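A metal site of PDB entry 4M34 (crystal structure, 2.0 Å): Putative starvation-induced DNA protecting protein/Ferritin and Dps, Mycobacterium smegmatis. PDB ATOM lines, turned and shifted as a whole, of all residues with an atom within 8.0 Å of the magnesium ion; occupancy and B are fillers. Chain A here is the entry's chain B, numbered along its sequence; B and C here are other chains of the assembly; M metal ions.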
ATOM      1  N   SER A  54       3.409  20.001 -19.784  1.00  0.00           N
ATOM      2  CA  SER A  54       2.144  20.073 -19.045  1.00  0.00           C
ATOM      3  C   SER A  54       1.142  19.015 -19.495  1.00  0.00           C
ATOM      4  O   SER A  54       0.834  18.903 -20.676  1.00  0.00           O
ATOM      5  CB  SER A  54       1.539  21.465 -19.177  1.00  0.00           C
ATOM      6  OG  SER A  54       2.468  22.449 -18.751  1.00  0.00           O
ATOM      7  N   ASN A  55       0.651  18.245 -18.526  1.00  0.00           N
ATOM      8  CA  ASN A  55      -0.279  17.134 -18.763  1.00  0.00           C
ATOM      9  C   ASN A  55       0.348  15.986 -19.561  1.00  0.00           C
ATOM     10  O   ASN A  55      -0.327  15.309 -20.357  1.00  0.00           O
ATOM     11  CB  ASN A  55      -1.588  17.607 -19.400  1.00  0.00           C
ATOM     12  CG  ASN A  55      -2.742  16.662 -19.118  1.00  0.00           C
ATOM     13  OD1 ASN A  55      -2.732  15.955 -18.110  1.00  0.00           O
ATOM     14  ND2 ASN A  55      -3.729  16.636 -20.005  1.00  0.00           N
ATOM     15  N   PHE A  56       1.649  15.776 -19.349  1.00  0.00           N
ATOM     16  CA  PHE A  56       2.374  14.670 -19.961  1.00  0.00           C
ATOM     17  C   PHE A  56       1.646  13.328 -19.833  1.00  0.00           C
ATOM     18  O   PHE A  56       1.528  12.594 -20.805  1.00  0.00           O
ATOM     19  CB  PHE A  56       3.771  14.528 -19.336  1.00  0.00           C
ATOM     20  CG  PHE A  56       4.387  13.176 -19.550  1.00  0.00           C
ATOM     21  CD1 PHE A  56       4.997  12.866 -20.761  1.00  0.00           C
ATOM     22  CD2 PHE A  56       4.329  12.199 -18.561  1.00  0.00           C
ATOM     23  CE1 PHE A  56       5.560  11.600 -20.979  1.00  0.00           C
ATOM     24  CE2 PHE A  56       4.889  10.938 -18.772  1.00  0.00           C
ATOM     25  CZ  PHE A  56       5.501  10.645 -19.980  1.00  0.00           C
ATOM     26  N   ARG A  57       1.199  13.020 -18.622  1.00  0.00           N
ATOM     27  CA  ARG A  57       0.722  11.676 -18.296  1.00  0.00           C
ATOM     28  C   ARG A  57      -0.537  11.301 -19.079  1.00  0.00           C
ATOM     29  O   ARG A  57      -0.598  10.213 -19.659  1.00  0.00           O
ATOM     30  CB  ARG A  57       0.522  11.510 -16.794  1.00  0.00           C
ATOM     31  CG  ARG A  57       0.146  10.095 -16.386  1.00  0.00           C
ATOM     32  CD  ARG A  57       0.104   9.944 -14.870  1.00  0.00           C
ATOM     33  NE  ARG A  57      -0.247   8.575 -14.481  1.00  0.00           N
ATOM     34  CZ  ARG A  57      -1.490   8.124 -14.378  1.00  0.00           C
ATOM     35  NH1 ARG A  57      -2.527   8.918 -14.635  1.00  0.00           N
ATOM     36  NH2 ARG A  57      -1.710   6.864 -14.013  1.00  0.00           N
ATOM     37  N   ASP A  58      -1.514  12.200 -19.107  1.00  0.00           N
ATOM     38  CA  ASP A  58      -2.743  11.992 -19.883  1.00  0.00           C
ATOM     39  C   ASP A  58      -2.471  11.720 -21.356  1.00  0.00           C
ATOM     40  O   ASP A  58      -3.080  10.820 -21.946  1.00  0.00           O
ATOM     41  CB  ASP A  58      -3.702  13.173 -19.743  1.00  0.00           C
ATOM     42  CG  ASP A  58      -4.680  13.013 -18.598  1.00  0.00           C
ATOM     43  OD1 ASP A  58      -5.162  11.892 -18.359  1.00  0.00           O
ATOM     44  OD2 ASP A  58      -4.977  14.033 -17.947  1.00  0.00           O
ATOM     45  N   LEU A  59      -1.587  12.515 -21.963  1.00  0.00           N
ATOM     46  CA  LEU A  59      -1.209  12.328 -23.365  1.00  0.00           C
ATOM     47  C   LEU A  59      -0.493  11.003 -23.588  1.00  0.00           C
ATOM     48  O   LEU A  59      -0.833  10.269 -24.498  1.00  0.00           O
ATOM     49  CB  LEU A  59      -0.348  13.489 -23.878  1.00  0.00           C
ATOM     50  CG  LEU A  59      -1.025  14.608 -24.675  1.00  0.00           C
ATOM     51  CD1 LEU A  59      -1.679  14.056 -25.945  1.00  0.00           C
ATOM     52  CD2 LEU A  59      -2.048  15.376 -23.823  1.00  0.00           C
ATOM     53  N   LEU A  61      -0.707   8.316 -21.814  1.00  0.00           N
ATOM     54  CA  LEU A  61      -1.709   7.244 -21.698  1.00  0.00           C
ATOM     55  C   LEU A  61      -2.698   7.196 -22.869  1.00  0.00           C
ATOM     56  O   LEU A  61      -2.988   6.120 -23.384  1.00  0.00           O
ATOM     57  CB  LEU A  61      -2.444   7.333 -20.359  1.00  0.00           C
ATOM     58  CG  LEU A  61      -1.628   7.060 -19.094  1.00  0.00           C
ATOM     59  CD1 LEU A  61      -2.444   7.388 -17.838  1.00  0.00           C
ATOM     60  CD2 LEU A  61      -1.107   5.612 -19.043  1.00  0.00           C
ATOM     61  N   GLU A 164      -7.724  18.783 -25.444  1.00  0.00           N
ATOM     62  CA  GLU A 164      -6.664  19.370 -24.614  1.00  0.00           C
ATOM     63  C   GLU A 164      -6.299  20.812 -25.032  1.00  0.00           C
ATOM     64  O   GLU A 164      -6.035  21.650 -24.176  1.00  0.00           O
ATOM     65  CB  GLU A 164      -5.424  18.471 -24.617  1.00  0.00           C
ATOM     66  CG  GLU A 164      -4.185  19.052 -23.917  1.00  0.00           C
ATOM     67  CD  GLU A 164      -4.298  19.095 -22.397  1.00  0.00           C
ATOM     68  OE1 GLU A 164      -3.599  19.917 -21.777  1.00  0.00           O
ATOM     69  OE2 GLU A 164      -5.079  18.308 -21.825  1.00  0.00           O
ATOM     70  N   SER B  54      -2.761  22.485 -10.992  1.00  0.00           N
ATOM     71  CA  SER B  54      -2.889  22.068 -12.389  1.00  0.00           C
ATOM     72  C   SER B  54      -2.374  20.651 -12.620  1.00  0.00           C
ATOM     73  O   SER B  54      -1.228  20.333 -12.293  1.00  0.00           O
ATOM     74  CB  SER B  54      -2.172  23.071 -13.304  1.00  0.00           C
ATOM     75  OG  SER B  54      -2.173  22.632 -14.652  1.00  0.00           O
ATOM     76  N   ASN B  55      -3.247  19.798 -13.171  1.00  0.00           N
ATOM     77  CA  ASN B  55      -2.956  18.381 -13.404  1.00  0.00           C
ATOM     78  C   ASN B  55      -2.792  17.551 -12.124  1.00  0.00           C
ATOM     79  O   ASN B  55      -2.011  16.592 -12.084  1.00  0.00           O
ATOM     80  CB  ASN B  55      -1.765  18.178 -14.348  1.00  0.00           C
ATOM     81  CG  ASN B  55      -1.806  16.829 -15.054  1.00  0.00           C
ATOM     82  OD1 ASN B  55      -2.887  16.272 -15.242  1.00  0.00           O
ATOM     83  ND2 ASN B  55      -0.647  16.310 -15.440  1.00  0.00           N
ATOM     84  N   PHE B  56      -3.561  17.922 -11.095  1.00  0.00           N
ATOM     85  CA  PHE B  56      -3.609  17.210  -9.826  1.00  0.00           C
ATOM     86  C   PHE B  56      -3.806  15.692  -9.989  1.00  0.00           C
ATOM     87  O   PHE B  56      -3.068  14.907  -9.400  1.00  0.00           O
ATOM     88  CB  PHE B  56      -4.732  17.756  -8.938  1.00  0.00           C
ATOM     89  CG  PHE B  56      -5.207  16.784  -7.878  1.00  0.00           C
ATOM     90  CD1 PHE B  56      -4.520  16.662  -6.684  1.00  0.00           C
ATOM     91  CD2 PHE B  56      -6.341  15.997  -8.093  1.00  0.00           C
ATOM     92  CE1 PHE B  56      -4.941  15.767  -5.702  1.00  0.00           C
ATOM     93  CE2 PHE B  56      -6.764  15.086  -7.127  1.00  0.00           C
ATOM     94  CZ  PHE B  56      -6.068  14.969  -5.932  1.00  0.00           C
ATOM     95  N   ARG B  57      -4.801  15.308 -10.783  1.00  0.00           N
ATOM     96  CA  ARG B  57      -5.231  13.915 -10.842  1.00  0.00           C
ATOM     97  C   ARG B  57      -4.132  12.976 -11.349  1.00  0.00           C
ATOM     98  O   ARG B  57      -3.871  11.943 -10.741  1.00  0.00           O
ATOM     99  CB  ARG B  57      -6.514  13.766 -11.669  1.00  0.00           C
ATOM    100  CG  ARG B  57      -7.121  12.371 -11.655  1.00  0.00           C
ATOM    101  CD  ARG B  57      -8.417  12.327 -12.431  1.00  0.00           C
ATOM    102  NE  ARG B  57      -8.986  10.981 -12.457  1.00  0.00           N
ATOM    103  CZ  ARG B  57      -8.719  10.057 -13.367  1.00  0.00           C
ATOM    104  NH1 ARG B  57      -7.876  10.315 -14.370  1.00  0.00           N
ATOM    105  NH2 ARG B  57      -9.299   8.868 -13.297  1.00  0.00           N
ATOM    106  N   ASP B  58      -3.482  13.365 -12.453  1.00  0.00           N
ATOM    107  CA  ASP B  58      -2.372  12.580 -13.007  1.00  0.00           C
ATOM    108  C   ASP B  58      -1.259  12.366 -11.977  1.00  0.00           C
ATOM    109  O   ASP B  58      -0.750  11.244 -11.839  1.00  0.00           O
ATOM    110  CB  ASP B  58      -1.779  13.268 -14.247  1.00  0.00           C
ATOM    111  CG  ASP B  58      -2.399  12.767 -15.535  1.00  0.00           C
ATOM    112  OD1 ASP B  58      -2.748  11.570 -15.636  1.00  0.00           O
ATOM    113  OD2 ASP B  58      -2.522  13.591 -16.468  1.00  0.00           O
ATOM    114  N   LEU B  59      -0.889  13.427 -11.272  1.00  0.00           N
ATOM    115  CA  LEU B  59       0.158  13.331 -10.249  1.00  0.00           C
ATOM    116  C   LEU B  59      -0.276  12.455  -9.092  1.00  0.00           C
ATOM    117  O   LEU B  59       0.466  11.573  -8.669  1.00  0.00           O
ATOM    118  CB  LEU B  59       0.579  14.721  -9.753  1.00  0.00           C
ATOM    119  CG  LEU B  59       1.812  15.349 -10.432  1.00  0.00           C
ATOM    120  CD1 LEU B  59       3.051  14.481 -10.236  1.00  0.00           C
ATOM    121  CD2 LEU B  59       1.563  15.631 -11.927  1.00  0.00           C
ATOM    122  N   LEU B  61      -2.456  10.055  -9.108  1.00  0.00           N
ATOM    123  CA  LEU B  61      -2.457   8.663  -9.560  1.00  0.00           C
ATOM    124  C   LEU B  61      -1.050   8.089  -9.779  1.00  0.00           C
ATOM    125  O   LEU B  61      -0.772   6.957  -9.343  1.00  0.00           O
ATOM    126  CB  LEU B  61      -3.292   8.514 -10.836  1.00  0.00           C
ATOM    127  CG  LEU B  61      -4.812   8.749 -10.715  1.00  0.00           C
ATOM    128  CD1 LEU B  61      -5.433   8.816 -12.099  1.00  0.00           C
ATOM    129  CD2 LEU B  61      -5.481   7.666  -9.866  1.00  0.00           C
ATOM    130  N   GLU B 164       6.359  16.139 -16.739  1.00  0.00           N
ATOM    131  CA  GLU B 164       5.356  17.176 -16.510  1.00  0.00           C
ATOM    132  C   GLU B 164       5.945  18.596 -16.485  1.00  0.00           C
ATOM    133  O   GLU B 164       5.323  19.533 -16.991  1.00  0.00           O
ATOM    134  CB  GLU B 164       4.605  16.885 -15.197  1.00  0.00           C
ATOM    135  CG  GLU B 164       3.668  18.001 -14.692  1.00  0.00           C
ATOM    136  CD  GLU B 164       2.385  18.153 -15.515  1.00  0.00           C
ATOM    137  OE1 GLU B 164       1.813  19.264 -15.494  1.00  0.00           O
ATOM    138  OE2 GLU B 164       1.952  17.180 -16.153  1.00  0.00           O
ATOM    139  N   SER C  54      -7.228  22.603 -21.060  1.00  0.00           N
ATOM    140  CA  SER C  54      -6.090  22.078 -20.315  1.00  0.00           C
ATOM    141  C   SER C  54      -6.499  21.010 -19.301  1.00  0.00           C
ATOM    142  O   SER C  54      -7.362  21.239 -18.466  1.00  0.00           O
ATOM    143  CB  SER C  54      -5.365  23.235 -19.597  1.00  0.00           C
ATOM    144  OG  SER C  54      -4.295  22.766 -18.804  1.00  0.00           O
ATOM    145  N   ASN C  55      -5.854  19.842 -19.405  1.00  0.00           N
ATOM    146  CA  ASN C  55      -6.165  18.670 -18.573  1.00  0.00           C
ATOM    147  C   ASN C  55      -7.572  18.082 -18.804  1.00  0.00           C
ATOM    148  O   ASN C  55      -8.217  17.597 -17.866  1.00  0.00           O
ATOM    149  CB  ASN C  55      -5.897  18.906 -17.080  1.00  0.00           C
ATOM    150  CG  ASN C  55      -5.613  17.620 -16.331  1.00  0.00           C
ATOM    151  OD1 ASN C  55      -5.184  16.636 -16.930  1.00  0.00           O
ATOM    152  ND2 ASN C  55      -5.861  17.613 -15.022  1.00  0.00           N
ATOM    153  N   PHE C  56      -8.024  18.130 -20.057  1.00  0.00           N
ATOM    154  CA  PHE C  56      -9.303  17.540 -20.459  1.00  0.00           C
ATOM    155  C   PHE C  56      -9.488  16.101 -19.984  1.00  0.00           C
ATOM    156  O   PHE C  56     -10.498  15.774 -19.363  1.00  0.00           O
ATOM    157  CB  PHE C  56      -9.475  17.603 -21.991  1.00  0.00           C
ATOM    158  CG  PHE C  56     -10.501  16.623 -22.530  1.00  0.00           C
ATOM    159  CD1 PHE C  56     -10.103  15.412 -23.096  1.00  0.00           C
ATOM    160  CD2 PHE C  56     -11.855  16.925 -22.465  1.00  0.00           C
ATOM    161  CE1 PHE C  56     -11.050  14.506 -23.582  1.00  0.00           C
ATOM    162  CE2 PHE C  56     -12.808  16.031 -22.950  1.00  0.00           C
ATOM    163  CZ  PHE C  56     -12.400  14.825 -23.514  1.00  0.00           C
ATOM    164  N   ARG C  57      -8.505  15.244 -20.279  1.00  0.00           N
ATOM    165  CA  ARG C  57      -8.648  13.805 -20.080  1.00  0.00           C
ATOM    166  C   ARG C  57      -8.907  13.424 -18.616  1.00  0.00           C
ATOM    167  O   ARG C  57      -9.818  12.647 -18.332  1.00  0.00           O
ATOM    168  CB  ARG C  57      -7.447  13.043 -20.646  1.00  0.00           C
ATOM    169  CG  ARG C  57      -7.630  11.521 -20.657  1.00  0.00           C
ATOM    170  CD  ARG C  57      -6.463  10.821 -21.344  1.00  0.00           C
ATOM    171  NE  ARG C  57      -6.609   9.368 -21.306  1.00  0.00           N
ATOM    172  CZ  ARG C  57      -6.169   8.592 -20.321  1.00  0.00           C
ATOM    173  NH1 ARG C  57      -5.564   9.120 -19.253  1.00  0.00           N
ATOM    174  NH2 ARG C  57      -6.355   7.273 -20.379  1.00  0.00           N
ATOM    175  N   ASP C  58      -8.107  13.989 -17.700  1.00  0.00           N
ATOM    176  CA  ASP C  58      -8.289  13.737 -16.261  1.00  0.00           C
ATOM    177  C   ASP C  58      -9.692  14.107 -15.787  1.00  0.00           C
ATOM    178  O   ASP C  58     -10.301  13.367 -15.023  1.00  0.00           O
ATOM    179  CB  ASP C  58      -7.282  14.529 -15.437  1.00  0.00           C
ATOM    180  CG  ASP C  58      -6.022  13.744 -15.119  1.00  0.00           C
ATOM    181  OD1 ASP C  58      -6.092  12.510 -14.947  1.00  0.00           O
ATOM    182  OD2 ASP C  58      -4.959  14.391 -15.025  1.00  0.00           O
ATOM    183  N   LEU C  59     -10.189  15.260 -16.249  1.00  0.00           N
ATOM    184  CA  LEU C  59     -11.521  15.726 -15.884  1.00  0.00           C
ATOM    185  C   LEU C  59     -12.607  14.868 -16.494  1.00  0.00           C
ATOM    186  O   LEU C  59     -13.548  14.475 -15.821  1.00  0.00           O
ATOM    187  CB  LEU C  59     -11.716  17.200 -16.252  1.00  0.00           C
ATOM    188  CG  LEU C  59     -11.454  18.247 -15.162  1.00  0.00           C
ATOM    189  CD1 LEU C  59     -12.306  17.978 -13.910  1.00  0.00           C
ATOM    190  CD2 LEU C  59      -9.972  18.340 -14.810  1.00  0.00           C
ATOM    191  N   GLU C 164      -7.705  20.491  -8.797  1.00  0.00           N
ATOM    192  CA  GLU C 164      -7.231  20.999 -10.089  1.00  0.00           C
ATOM    193  C   GLU C 164      -7.093  22.533 -10.107  1.00  0.00           C
ATOM    194  O   GLU C 164      -6.120  23.055 -10.657  1.00  0.00           O
ATOM    195  CB  GLU C 164      -8.173  20.540 -11.221  1.00  0.00           C
ATOM    196  CG  GLU C 164      -7.873  21.116 -12.615  1.00  0.00           C
ATOM    197  CD  GLU C 164      -6.560  20.621 -13.216  1.00  0.00           C
ATOM    198  OE1 GLU C 164      -6.133  19.476 -12.907  1.00  0.00           O
ATOM    199  OE2 GLU C 164      -5.955  21.378 -14.006  1.00  0.00           O
HETATM  200 MG    MG M   1      -3.841  15.133 -16.584  1.00  0.00          MG
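The side-chain amide nitrogen (ND2) of Asn 55 of chain C lies within hydrogen-bond range of the side-chain carboxylate (OE1) of Glu 164 of chain C, at 2.8 Å. The backbone NH (N) of Asn 55 of chain A sits at hydrogen-bond distance from the side-chain carboxylate (OE2) of Glu 164 of chain B (2.9 Å). OE2 of Glu 164 of chain B lies within hydrogen-bond range of ND2 of Asn 55 of chain B (2.8 Å). OD1 of Asp 58 of chain A is in salt-bridge range of NH1 of Arg 57 of chain C (2.9 Å). OE2 of Glu 164 of chain A sits at hydrogen-bond distance from N of Asn 55 of chain C, 3.0 Å away. The side-chain amide nitrogen (ND2) of Asn 55 of chain A is in hydrogen-bond range of the side-chain carboxylate (OE2) of Glu 164 of chain A (2.8 Å). The side-chain carboxylate (OD1) of Asp 58 of chain B lies within salt-bridge range of the guanidinium group (NH1) of Arg 57 of chain A, at 2.8 Å. The backbone NH of Asn 55 of chain B sits at hydrogen-bond distance from the side-chain carboxylate of Glu 164 of chain C, 2.9 Å away.
Six residues have an atom within 4 Å of the magnesium ion: Asn 55 of chain A, Asp 58 of chain A, Asn 55 of chain B, Asp 58 of chain B, Asn 55 of chain C and Asp 58 of chain C. Along chain A the residues within 4 Å of the magnesium ion span positions 55 to 58.
The magnesium ion is bound by the side-chain amide oxygen (OD1) of Asn 55 of chain B (2.0 Å), the side-chain carboxylate (OD2) of Asp 58 of chain B (2.0 Å), the side-chain amide oxygen (OD1) of Asn 55 of chain C (2.0 Å), the side-chain amide oxygen (OD1) of Asn 55 of chain A (2.1 Å), the side-chain carboxylate (OD2) of Asp 58 of chain C (2.1 Å) and the side-chain carboxylate (OD2) of Asp 58 of chain A (2.1 Å).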
